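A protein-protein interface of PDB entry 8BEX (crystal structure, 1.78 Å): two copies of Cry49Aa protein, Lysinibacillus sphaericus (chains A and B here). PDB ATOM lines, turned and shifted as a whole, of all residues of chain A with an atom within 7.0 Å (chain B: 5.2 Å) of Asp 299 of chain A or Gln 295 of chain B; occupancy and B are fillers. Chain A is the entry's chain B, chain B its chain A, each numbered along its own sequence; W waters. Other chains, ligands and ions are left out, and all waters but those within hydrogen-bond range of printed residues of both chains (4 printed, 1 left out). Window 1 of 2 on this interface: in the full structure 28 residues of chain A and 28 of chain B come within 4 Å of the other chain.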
ATOM      1  N   ASN A   3      10.756  29.340 -15.017  1.00  0.00           N
ATOM      2  CA  ASN A   3      11.734  29.006 -16.078  1.00  0.00           C
ATOM      3  C   ASN A   3      11.063  28.110 -17.113  1.00  0.00           C
ATOM      4  O   ASN A   3      11.595  27.011 -17.341  1.00  0.00           O
ATOM      5  CB  ASN A   3      12.920  28.255 -15.464  1.00  0.00           C
ATOM      6  CG  ASN A   3      14.251  28.861 -15.816  1.00  0.00           C
ATOM      7  OD1 ASN A   3      14.393  29.512 -16.854  1.00  0.00           O
ATOM      8  ND2 ASN A   3      15.208  28.662 -14.918  1.00  0.00           N
ATOM      9  N   LEU A   4       9.907  28.508 -17.655  1.00  0.00           N
ATOM     10  CA  LEU A   4       9.140  27.650 -18.589  1.00  0.00           C
ATOM     11  C   LEU A   4       8.924  28.381 -19.909  1.00  0.00           C
ATOM     12  O   LEU A   4       8.783  29.604 -19.946  1.00  0.00           O
ATOM     13  CB  LEU A   4       7.784  27.261 -17.990  1.00  0.00           C
ATOM     14  CG  LEU A   4       7.795  26.159 -16.936  1.00  0.00           C
ATOM     15  CD1 LEU A   4       6.399  25.985 -16.362  1.00  0.00           C
ATOM     16  CD2 LEU A   4       8.295  24.840 -17.521  1.00  0.00           C
ATOM     17  N   ALA A  70       6.597  20.602 -20.736  1.00  0.00           N
ATOM     18  CA  ALA A  70       8.034  20.569 -21.101  1.00  0.00           C
ATOM     19  C   ALA A  70       8.726  19.419 -20.373  1.00  0.00           C
ATOM     20  O   ALA A  70       8.761  19.413 -19.056  1.00  0.00           O
ATOM     21  CB  ALA A  70       8.691  21.880 -20.758  1.00  0.00           C
ATOM     22  N   LEU A  71       9.282  18.494 -21.150  1.00  0.00           N
ATOM     23  CA  LEU A  71      10.138  17.392 -20.632  1.00  0.00           C
ATOM     24  C   LEU A  71      11.586  17.870 -20.495  1.00  0.00           C
ATOM     25  O   LEU A  71      12.003  18.919 -21.138  1.00  0.00           O
ATOM     26  CB  LEU A  71      10.050  16.178 -21.566  1.00  0.00           C
ATOM     27  CG  LEU A  71       8.645  15.706 -21.929  1.00  0.00           C
ATOM     28  CD1 LEU A  71       8.699  14.453 -22.757  1.00  0.00           C
ATOM     29  CD2 LEU A  71       7.830  15.428 -20.701  1.00  0.00           C
ATOM     30  N   ASP A  72      12.353  17.133 -19.686  1.00  0.00           N
ATOM     31  CA  ASP A  72      13.794  17.376 -19.464  1.00  0.00           C
ATOM     32  C   ASP A  72      14.569  17.327 -20.790  1.00  0.00           C
ATOM     33  O   ASP A  72      15.651  17.994 -20.895  1.00  0.00           O
ATOM     34  CB  ASP A  72      14.353  16.331 -18.497  1.00  0.00           C
ATOM     35  CG  ASP A  72      13.896  16.439 -17.038  1.00  0.00           C
ATOM     36  OD1 ASP A  72      13.247  17.469 -16.670  1.00  0.00           O
ATOM     37  OD2 ASP A  72      14.280  15.510 -16.262  1.00  0.00           O
ATOM     38  N   ASN A  73      14.113  16.516 -21.746  1.00  0.00           N
ATOM     39  CA  ASN A  73      14.840  16.283 -23.033  1.00  0.00           C
ATOM     40  C   ASN A  73      14.445  17.307 -24.109  1.00  0.00           C
ATOM     41  O   ASN A  73      14.867  17.140 -25.277  1.00  0.00           O
ATOM     42  CB  ASN A  73      14.662  14.855 -23.527  1.00  0.00           C
ATOM     43  CG  ASN A  73      13.238  14.500 -23.891  1.00  0.00           C
ATOM     44  OD1 ASN A  73      12.343  15.347 -24.007  1.00  0.00           O
ATOM     45  ND2 ASN A  73      13.013  13.217 -24.087  1.00  0.00           N
ATOM     46  N   ASN A  74      13.714  18.360 -23.753  1.00  0.00           N
ATOM     47  CA  ASN A  74      13.332  19.482 -24.668  1.00  0.00           C
ATOM     48  C   ASN A  74      12.201  19.060 -25.614  1.00  0.00           C
ATOM     49  O   ASN A  74      11.827  19.884 -26.505  1.00  0.00           O
ATOM     50  CB  ASN A  74      14.473  20.044 -25.526  1.00  0.00           C
ATOM     51  CG  ASN A  74      14.234  21.510 -25.867  1.00  0.00           C
ATOM     52  OD1 ASN A  74      13.700  22.267 -25.041  1.00  0.00           O
ATOM     53  ND2 ASN A  74      14.592  21.936 -27.070  1.00  0.00           N
ATOM     54  N   GLY A 204      12.065  24.347  -0.987  1.00  0.00           N
ATOM     55  CA  GLY A 204      11.869  24.264  -2.433  1.00  0.00           C
ATOM     56  C   GLY A 204      10.419  24.077  -2.785  1.00  0.00           C
ATOM     57  O   GLY A 204       9.584  23.717  -1.912  1.00  0.00           O
ATOM     58  N   ARG A 205      10.111  24.316  -4.050  1.00  0.00           N
ATOM     59  CA  ARG A 205       8.755  24.074  -4.570  1.00  0.00           C
ATOM     60  C   ARG A 205       8.867  23.907  -6.077  1.00  0.00           C
ATOM     61  O   ARG A 205       9.696  24.620  -6.715  1.00  0.00           O
ATOM     62  CB  ARG A 205       7.801  25.202  -4.143  1.00  0.00           C
ATOM     63  CG  ARG A 205       8.008  26.540  -4.830  1.00  0.00           C
ATOM     64  CD  ARG A 205       9.193  27.277  -4.274  1.00  0.00           C
ATOM     65  NE  ARG A 205       9.124  28.679  -4.615  1.00  0.00           N
ATOM     66  CZ  ARG A 205       9.778  29.273  -5.609  1.00  0.00           C
ATOM     67  NH1 ARG A 205      10.567  28.582  -6.412  1.00  0.00           N
ATOM     68  NH2 ARG A 205       9.604  30.563  -5.822  1.00  0.00           N
ATOM     69  N   THR A 206       8.023  23.043  -6.622  1.00  0.00           N
ATOM     70  CA  THR A 206       7.998  22.749  -8.075  1.00  0.00           C
ATOM     71  C   THR A 206       6.555  22.563  -8.529  1.00  0.00           C
ATOM     72  O   THR A 206       5.686  22.106  -7.716  1.00  0.00           O
ATOM     73  CB  THR A 206       8.833  21.493  -8.377  1.00  0.00           C
ATOM     74  OG1 THR A 206       8.995  21.393  -9.792  1.00  0.00           O
ATOM     75  CG2 THR A 206       8.220  20.228  -7.825  1.00  0.00           C
ATOM     76  N   PHE A 293      10.215  14.207 -16.169  1.00  0.00           N
ATOM     77  CA  PHE A 293      10.305  15.548 -15.540  1.00  0.00           C
ATOM     78  C   PHE A 293      11.309  15.599 -14.382  1.00  0.00           C
ATOM     79  O   PHE A 293      11.337  16.656 -13.656  1.00  0.00           O
ATOM     80  CB  PHE A 293       8.933  15.950 -15.009  1.00  0.00           C
ATOM     81  CG  PHE A 293       7.849  15.938 -16.060  1.00  0.00           C
ATOM     82  CD1 PHE A 293       7.642  17.042 -16.867  1.00  0.00           C
ATOM     83  CD2 PHE A 293       7.050  14.818 -16.253  1.00  0.00           C
ATOM     84  CE1 PHE A 293       6.643  17.031 -17.843  1.00  0.00           C
ATOM     85  CE2 PHE A 293       6.064  14.809 -17.243  1.00  0.00           C
ATOM     86  CZ  PHE A 293       5.868  15.913 -18.038  1.00  0.00           C
ATOM     87  N   ARG A 294      12.094  14.533 -14.169  1.00  0.00           N
ATOM     88  CA  ARG A 294      12.812  14.328 -12.878  1.00  0.00           C
ATOM     89  C   ARG A 294      13.800  15.470 -12.603  1.00  0.00           C
ATOM     90  O   ARG A 294      13.890  15.890 -11.414  1.00  0.00           O
ATOM     91  CB  ARG A 294      13.480  12.950 -12.822  1.00  0.00           C
ATOM     92  CG  ARG A 294      14.520  12.651 -13.887  1.00  0.00           C
ATOM     93  CD  ARG A 294      15.090  11.259 -13.626  1.00  0.00           C
ATOM     94  NE  ARG A 294      15.797  11.314 -12.362  1.00  0.00           N
ATOM     95  CZ  ARG A 294      15.939  10.318 -11.502  1.00  0.00           C
ATOM     96  NH1 ARG A 294      16.572  10.550 -10.370  1.00  0.00           N
ATOM     97  NH2 ARG A 294      15.434   9.123 -11.747  1.00  0.00           N
ATOM     98  N   GLN A 295      14.551  15.946 -13.603  1.00  0.00           N
ATOM     99  CA  GLN A 295      15.623  16.946 -13.342  1.00  0.00           C
ATOM    100  C   GLN A 295      14.981  18.294 -12.979  1.00  0.00           C
ATOM    101  O   GLN A 295      15.519  18.993 -12.084  1.00  0.00           O
ATOM    102  CB  GLN A 295      16.629  17.096 -14.483  1.00  0.00           C
ATOM    103  CG  GLN A 295      17.855  17.902 -14.085  1.00  0.00           C
ATOM    104  CD  GLN A 295      18.666  17.206 -13.007  1.00  0.00           C
ATOM    105  OE1 GLN A 295      19.016  16.028 -13.125  1.00  0.00           O
ATOM    106  NE2 GLN A 295      18.944  17.919 -11.920  1.00  0.00           N
ATOM    107  N   GLN A 296      13.878  18.674 -13.642  1.00  0.00           N
ATOM    108  CA  GLN A 296      13.127  19.914 -13.272  1.00  0.00           C
ATOM    109  C   GLN A 296      12.623  19.787 -11.835  1.00  0.00           C
ATOM    110  O   GLN A 296      12.744  20.795 -11.071  1.00  0.00           O
ATOM    111  CB  GLN A 296      11.946  20.174 -14.221  1.00  0.00           C
ATOM    112  CG  GLN A 296      12.409  20.567 -15.605  1.00  0.00           C
ATOM    113  CD  GLN A 296      11.264  20.555 -16.588  1.00  0.00           C
ATOM    114  OE1 GLN A 296      10.493  21.535 -16.688  1.00  0.00           O
ATOM    115  NE2 GLN A 296      11.128  19.445 -17.313  1.00  0.00           N
ATOM    116  N   ILE A 297      12.053  18.634 -11.484  1.00  0.00           N
ATOM    117  CA  ILE A 297      11.466  18.400 -10.130  1.00  0.00           C
ATOM    118  C   ILE A 297      12.568  18.527  -9.071  1.00  0.00           C
ATOM    119  O   ILE A 297      12.380  19.289  -8.068  1.00  0.00           O
ATOM    120  CB  ILE A 297      10.718  17.059 -10.081  1.00  0.00           C
ATOM    121  CG1 ILE A 297       9.430  17.149 -10.908  1.00  0.00           C
ATOM    122  CG2 ILE A 297      10.436  16.636  -8.646  1.00  0.00           C
ATOM    123  CD1 ILE A 297       8.747  15.838 -11.117  1.00  0.00           C
ATOM    124  N   ILE A 298      13.724  17.899  -9.332  1.00  0.00           N
ATOM    125  CA  ILE A 298      14.912  17.960  -8.429  1.00  0.00           C
ATOM    126  C   ILE A 298      15.409  19.394  -8.279  1.00  0.00           C
ATOM    127  O   ILE A 298      15.657  19.829  -7.100  1.00  0.00           O
ATOM    128  CB  ILE A 298      15.990  17.005  -8.967  1.00  0.00           C
ATOM    129  CG1 ILE A 298      15.622  15.564  -8.601  1.00  0.00           C
ATOM    130  CG2 ILE A 298      17.373  17.374  -8.500  1.00  0.00           C
ATOM    131  CD1 ILE A 298      16.458  14.571  -9.366  1.00  0.00           C
ATOM    132  N   ASP A 299      15.628  20.090  -9.404  1.00  0.00           N
ATOM    133  CA  ASP A 299      16.230  21.448  -9.439  1.00  0.00           C
ATOM    134  C   ASP A 299      15.336  22.429  -8.667  1.00  0.00           C
ATOM    135  O   ASP A 299      15.877  23.245  -7.897  1.00  0.00           O
ATOM    136  CB  ASP A 299      16.504  21.916 -10.871  1.00  0.00           C
ATOM    137  CG  ASP A 299      17.674  21.195 -11.525  1.00  0.00           C
ATOM    138  OD1 ASP A 299      18.458  20.537 -10.759  1.00  0.00           O
ATOM    139  OD2 ASP A 299      17.810  21.286 -12.765  1.00  0.00           O
ATOM    140  N   ASN A 300      14.018  22.347  -8.843  1.00  0.00           N
ATOM    141  CA  ASN A 300      13.079  23.355  -8.288  1.00  0.00           C
ATOM    142  C   ASN A 300      12.734  23.015  -6.838  1.00  0.00           C
ATOM    143  O   ASN A 300      12.573  23.990  -6.031  1.00  0.00           O
ATOM    144  CB  ASN A 300      11.861  23.523  -9.196  1.00  0.00           C
ATOM    145  CG  ASN A 300      12.267  24.179 -10.495  1.00  0.00           C
ATOM    146  OD1 ASN A 300      12.801  25.275 -10.521  1.00  0.00           O
ATOM    147  ND2 ASN A 300      12.113  23.480 -11.589  1.00  0.00           N
ATOM    148  N   SER A 301      12.617  21.724  -6.499  1.00  0.00           N
ATOM    149  CA  SER A 301      12.242  21.255  -5.143  1.00  0.00           C
ATOM    150  C   SER A 301      13.473  21.247  -4.222  1.00  0.00           C
ATOM    151  O   SER A 301      13.274  21.092  -2.965  1.00  0.00           O
ATOM    152  CB  SER A 301      11.535  19.910  -5.187  1.00  0.00           C
ATOM    153  OG  SER A 301      12.408  18.799  -5.469  1.00  0.00           O
ATOM    154  N   ASN A 302      14.684  21.439  -4.763  1.00  0.00           N
ATOM    155  CA  ASN A 302      15.955  21.373  -3.970  1.00  0.00           C
ATOM    156  C   ASN A 302      16.009  20.047  -3.210  1.00  0.00           C
ATOM    157  O   ASN A 302      16.266  20.026  -1.938  1.00  0.00           O
ATOM    158  CB  ASN A 302      16.143  22.588  -3.046  1.00  0.00           C
ATOM    159  CG  ASN A 302      16.337  23.848  -3.853  1.00  0.00           C
ATOM    160  OD1 ASN A 302      17.135  23.857  -4.796  1.00  0.00           O
ATOM    161  ND2 ASN A 302      15.600  24.908  -3.530  1.00  0.00           N
ATOM    162  N   THR A 303      15.779  18.962  -3.945  1.00  0.00           N
ATOM    163  CA  THR A 303      15.998  17.557  -3.497  1.00  0.00           C
ATOM    164  C   THR A 303      17.120  16.965  -4.359  1.00  0.00           C
ATOM    165  O   THR A 303      17.749  17.741  -5.168  1.00  0.00           O
ATOM    166  CB  THR A 303      14.701  16.751  -3.570  1.00  0.00           C
ATOM    167  OG1 THR A 303      14.209  16.843  -4.918  1.00  0.00           O
ATOM    168  CG2 THR A 303      13.690  17.245  -2.554  1.00  0.00           C
ATOM    169  N   ASN B   3      22.986  21.893  -5.659  1.00  0.00           N
ATOM    170  CA  ASN B   3      21.985  20.800  -5.723  1.00  0.00           C
ATOM    171  C   ASN B   3      22.615  19.561  -6.343  1.00  0.00           C
ATOM    172  O   ASN B   3      22.045  19.068  -7.321  1.00  0.00           O
ATOM    173  CB  ASN B   3      20.793  21.241  -6.575  1.00  0.00           C
ATOM    174  CG  ASN B   3      19.467  21.060  -5.881  1.00  0.00           C
ATOM    175  OD1 ASN B   3      19.304  20.142  -5.076  1.00  0.00           O
ATOM    176  ND2 ASN B   3      18.539  21.959  -6.193  1.00  0.00           N
ATOM    177  N   ASP B  72      21.424  14.657 -16.547  1.00  0.00           N
ATOM    178  CA  ASP B  72      19.980  14.920 -16.348  1.00  0.00           C
ATOM    179  C   ASP B  72      19.202  13.602 -16.133  1.00  0.00           C
ATOM    180  O   ASP B  72      18.119  13.631 -15.479  1.00  0.00           O
ATOM    181  CB  ASP B  72      19.398  15.670 -17.559  1.00  0.00           C
ATOM    182  CG  ASP B  72      19.872  17.103 -17.766  1.00  0.00           C
ATOM    183  OD1 ASP B  72      20.532  17.678 -16.848  1.00  0.00           O
ATOM    184  OD2 ASP B  72      19.525  17.670 -18.842  1.00  0.00           O
ATOM    185  N   PHE B 293      23.582  17.512 -20.107  1.00  0.00           N
ATOM    186  CA  PHE B 293      23.467  18.411 -18.921  1.00  0.00           C
ATOM    187  C   PHE B 293      22.474  19.556 -19.147  1.00  0.00           C
ATOM    188  O   PHE B 293      22.438  20.480 -18.279  1.00  0.00           O
ATOM    189  CB  PHE B 293      24.825  19.026 -18.597  1.00  0.00           C
ATOM    190  CG  PHE B 293      25.910  18.007 -18.378  1.00  0.00           C
ATOM    191  CD1 PHE B 293      26.106  17.460 -17.120  1.00  0.00           C
ATOM    192  CD2 PHE B 293      26.744  17.614 -19.423  1.00  0.00           C
ATOM    193  CE1 PHE B 293      27.109  16.514 -16.915  1.00  0.00           C
ATOM    194  CE2 PHE B 293      27.733  16.662 -19.213  1.00  0.00           C
ATOM    195  CZ  PHE B 293      27.904  16.107 -17.962  1.00  0.00           C
ATOM    196  N   ARG B 294      21.691  19.520 -20.242  1.00  0.00           N
ATOM    197  CA  ARG B 294      20.953  20.717 -20.734  1.00  0.00           C
ATOM    198  C   ARG B 294      19.975  21.242 -19.679  1.00  0.00           C
ATOM    199  O   ARG B 294      19.891  22.500 -19.524  1.00  0.00           O
ATOM    200  CB  ARG B 294      20.255  20.454 -22.078  1.00  0.00           C
ATOM    201  CG  ARG B 294      19.219  19.339 -22.088  1.00  0.00           C
ATOM    202  CD  ARG B 294      18.505  19.268 -23.427  1.00  0.00           C
ATOM    203  NE  ARG B 294      17.802  20.523 -23.681  1.00  0.00           N
ATOM    204  CZ  ARG B 294      17.751  21.178 -24.851  1.00  0.00           C
ATOM    205  NH1 ARG B 294      18.320  20.687 -25.947  1.00  0.00           N
ATOM    206  NH2 ARG B 294      17.099  22.328 -24.920  1.00  0.00           N
ATOM    207  N   GLN B 295      19.219  20.373 -19.001  1.00  0.00           N
ATOM    208  CA  GLN B 295      18.144  20.830 -18.085  1.00  0.00           C
ATOM    209  C   GLN B 295      18.781  21.479 -16.857  1.00  0.00           C
ATOM    210  O   GLN B 295      18.234  22.517 -16.379  1.00  0.00           O
ATOM    211  CB  GLN B 295      17.150  19.734 -17.707  1.00  0.00           C
ATOM    212  CG  GLN B 295      15.919  20.278 -17.008  1.00  0.00           C
ATOM    213  CD  GLN B 295      15.099  21.160 -17.931  1.00  0.00           C
ATOM    214  OE1 GLN B 295      14.748  20.756 -19.050  1.00  0.00           O
ATOM    215  NE2 GLN B 295      14.797  22.371 -17.480  1.00  0.00           N
ATOM    216  N   GLN B 296      19.886  20.917 -16.338  1.00  0.00           N
ATOM    217  CA  GLN B 296      20.624  21.554 -15.203  1.00  0.00           C
ATOM    218  C   GLN B 296      21.127  22.940 -15.622  1.00  0.00           C
ATOM    219  O   GLN B 296      20.962  23.918 -14.818  1.00  0.00           O
ATOM    220  CB  GLN B 296      21.797  20.691 -14.730  1.00  0.00           C
ATOM    221  CG  GLN B 296      21.345  19.408 -14.074  1.00  0.00           C
ATOM    222  CD  GLN B 296      22.508  18.469 -13.868  1.00  0.00           C
ATOM    223  OE1 GLN B 296      23.298  18.635 -12.915  1.00  0.00           O
ATOM    224  NE2 GLN B 296      22.621  17.487 -14.761  1.00  0.00           N
ATOM    225  N   ILE B 297      21.688  23.045 -16.817  1.00  0.00           N
ATOM    226  CA  ILE B 297      22.271  24.319 -17.339  1.00  0.00           C
ATOM    227  C   ILE B 297      21.161  25.370 -17.469  1.00  0.00           C
ATOM    228  O   ILE B 297      21.316  26.497 -16.934  1.00  0.00           O
ATOM    229  CB  ILE B 297      23.060  24.069 -18.632  1.00  0.00           C
ATOM    230  CG1 ILE B 297      24.351  23.302 -18.313  1.00  0.00           C
ATOM    231  CG2 ILE B 297      23.335  25.380 -19.369  1.00  0.00           C
ATOM    232  CD1 ILE B 297      25.071  22.787 -19.537  1.00  0.00           C
ATOM    233  N   ILE B 298      20.026  24.981 -18.043  1.00  0.00           N
ATOM    234  CA  ILE B 298      18.831  25.865 -18.199  1.00  0.00           C
ATOM    235  C   ILE B 298      18.304  26.324 -16.837  1.00  0.00           C
ATOM    236  O   ILE B 298      18.043  27.583 -16.670  1.00  0.00           O
ATOM    237  CB  ILE B 298      17.771  25.115 -19.027  1.00  0.00           C
ATOM    238  CG1 ILE B 298      18.152  25.180 -20.503  1.00  0.00           C
ATOM    239  CG2 ILE B 298      16.378  25.628 -18.783  1.00  0.00           C
ATOM    240  CD1 ILE B 298      17.414  24.166 -21.310  1.00  0.00           C
ATOM    241  N   ASP B 299      18.077  25.374 -15.912  1.00  0.00           N
ATOM    242  CA  ASP B 299      17.464  25.652 -14.588  1.00  0.00           C
ATOM    243  C   ASP B 299      18.353  26.622 -13.788  1.00  0.00           C
ATOM    244  O   ASP B 299      17.816  27.538 -13.146  1.00  0.00           O
ATOM    245  CB  ASP B 299      17.192  24.349 -13.821  1.00  0.00           C
ATOM    246  CG  ASP B 299      16.033  23.544 -14.387  1.00  0.00           C
ATOM    247  OD1 ASP B 299      15.238  24.142 -15.207  1.00  0.00           O
ATOM    248  OD2 ASP B 299      15.910  22.349 -14.027  1.00  0.00           O
ATOM    249  N   ASN B 300      19.674  26.438 -13.820  1.00  0.00           N
ATOM    250  CA  ASN B 300      20.607  27.228 -12.975  1.00  0.00           C
ATOM    251  C   ASN B 300      20.956  28.568 -13.627  1.00  0.00           C
ATOM    252  O   ASN B 300      21.110  29.568 -12.857  1.00  0.00           O
ATOM    253  CB  ASN B 300      21.809  26.375 -12.614  1.00  0.00           C
ATOM    254  CG  ASN B 300      21.400  25.287 -11.652  1.00  0.00           C
ATOM    255  OD1 ASN B 300      20.950  25.588 -10.562  1.00  0.00           O
ATOM    256  ND2 ASN B 300      21.491  24.037 -12.053  1.00  0.00           N
HETATM  257  O   HOH W   1      15.862  13.616 -17.172  1.00  0.00           O
HETATM  258  O   HOH W   2      20.531  21.689 -10.109  1.00  0.00           O
HETATM  259  O   HOH W   3      15.837  20.590 -21.970  1.00  0.00           O
HETATM  260  O   HOH W   4      17.928  16.355 -20.450  1.00  0.00           O
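Asp 72 of chain A touches Arg 294 of chain B, but with the chains exchanged Arg 294 of chain A does not touch Asp 72 of chain B (4.1 Å). Asp 72 of chain A touches Gln 295 of chain B, and with the chains exchanged Gln 295 of chain A touches Asp 72 of chain B. Gln 295 of chain A touches Asp 299 of chain B, and with the chains exchanged Asp 299 of chain A touches Gln 295 of chain B. Asp 299 of chain B touches its own counterpart, Asp 299 of chain A. Of the 18 pairs that touch across the chains among the printed residues, 13 have their exchanged pair printed and touching as well.
The backbone carbonyl oxygen (O) of Gln 296 of chain B is in hydrogen-bond range of the side-chain amide nitrogen (ND2) of Asn 300 of chain B (2.8 Å). OD1 of Asp 72 of chain B lies within hydrogen-bond range of NE2 of Gln 296 of chain B (3.0 Å). The side-chain amide oxygen (OD1) of Asn 302 of chain A sits close to the backbone carbonyl oxygen (O) of Asp 299 of chain A (3.4 Å). The side-chain carboxylate (OD2) of Asp 72 of chain A lies within hydrogen-bond range of the backbone NH (N) of Gln 295 of chain A, 2.7 Å away. The backbone carbonyl oxygen (O) of Ile 298 of chain A is in hydrogen-bond range of the backbone NH (N) of Thr 303 of chain A. The side-chain amide nitrogen (NE2) of Gln 296 of chain A sits at hydrogen-bond distance from the side-chain carboxylate (OD1) of Asp 72 of chain A (3.0 Å).
Of the 10 printed residues of chain B, 7 touch a printed residue of chain A. Along chain B the printed residues that touch a printed residue of chain A span positions 3 to 299. Among the printed residues, no Asp or Glu carboxylate lies within 4 Å of a Lys or Arg side-chain nitrogen of the other chain.
Water W2 lies within hydrogen-bond range of the side-chain carboxylate (OD1) of Asp 299 of chain A (2.5 Å) and the side-chain amide nitrogen (ND2) of Asn 300 of chain B (3.2 Å). Water W3 lies within hydrogen-bond range of NE of Arg 294 of chain B (2.6 Å), O of Asp 72 of chain A (2.8 Å) and OE1 of Gln 295 of chain B (3.1 Å). Water W4 lies within hydrogen-bond range of the side-chain carboxylate of Asp 72 of chain B (2.6 Å) and the backbone carbonyl oxygen of Asp 72 of chain A (2.8 Å). Water W1 lies within hydrogen-bond range of OD2 of Asp 72 of chain A (2.6 Å) and O of Asp 72 of chain B (2.8 Å).
Printed residues of chain B within 4 Å of Leu 71 of chain A: Gln 295. Gly 204 of chain A touches none of the printed residues of chain B. Arg 294 of chain A touches none of the printed residues of chain B. Of the printed residues of chain B, Gln 295 of chain A touches Asp 72 (3.5 Å), Gln 296 (3.6 Å) and Asp 299 (3.9 Å). Printed residues of chain B within 4 Å of Asp 299 of chain A: Asn 3 (3.4 Å), Gln 295 (3.8 Å), Gln 296 (3.7 Å) and Asp 299 (2.5 Å). Printed residues of chain A within 4 Å of Asn 3 of chain B: Ile 298, Asp 299, Asn 302 and Thr 303. Of chain A, only Leu 71, Asp 72, Gln 296 and Asp 299 come within 4 Å of Gln 295 of chain B. Of the printed residues of chain A, Asp 299 of chain B touches Asn 3, Gln 295, Gln 296 and Asp 299. The nearest residue of chain B that does not touch Asp 299 of chain A is Asn 300 of chain B (4.7 Å). The nearest printed residue of chain A that does not touch Gln 296 of chain B is Asp 72 of chain A (6.9 Å).
Among the printed residues, pairs that only touch across the chains: Asn 3 of chain A with Ile 298 of chain B (3.5 Å), Leu 71 of chain A with Gln 295 of chain B (3.9 Å), Asp 72 of chain A with Arg 294 of chain B (3.995 Å), Gln 295 of chain A with Gln 296 of chain B (3.6 Å), Gln 295 of chain A with Asp 299 of chain B (3.9 Å), Gln 296 of chain A with Gln 295 of chain B (3.5 Å), Gln 296 of chain A with Asp 299 of chain B (3.8 Å), Ile 298 of chain A with Asn 3 of chain B (3.7 Å), Asp 299 of chain A with Gln 295 of chain B (3.8 Å) and Asp 299 of chain A with Gln 296 of chain B (3.7 Å).
The side-chain amide nitrogen (ND2) of Asn 3 of chain A lies within hydrogen-bond range of the backbone carbonyl oxygen (O) of Asp 299 of chain B, 3.3 Å away. ND2 of Asn 3 of chain B sits at hydrogen-bond distance from OD1 of Asn 302 of chain A, at 2.7 Å. The side-chain carboxylate (OD2) of Asp 299 of chain A sits close to the side-chain carboxylate (OD2) of Asp 299 of chain B, 2.5 Å away. The guanidinium group (NH2) of Arg 294 of chain B sits close to the side-chain amide nitrogen (ND2) of Asn 74 of chain A (3.3 Å). The side-chain amide oxygen (OE1) of Gln 295 of chain B sits close to the backbone carbonyl oxygen (O) of Asp 72 of chain A. The side-chain amide nitrogen (ND2) of Asn 3 of chain B is in hydrogen-bond range of the backbone carbonyl oxygen (O) of Asp 299 of chain A (3.4 Å). The backbone carbonyl oxygen of Asp 72 of chain B lies close to the side-chain amide oxygen of Gln 295 of chain A (3.5 Å). OD1 of Asn 3 of chain B lies close to O of Thr 303 of chain A.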
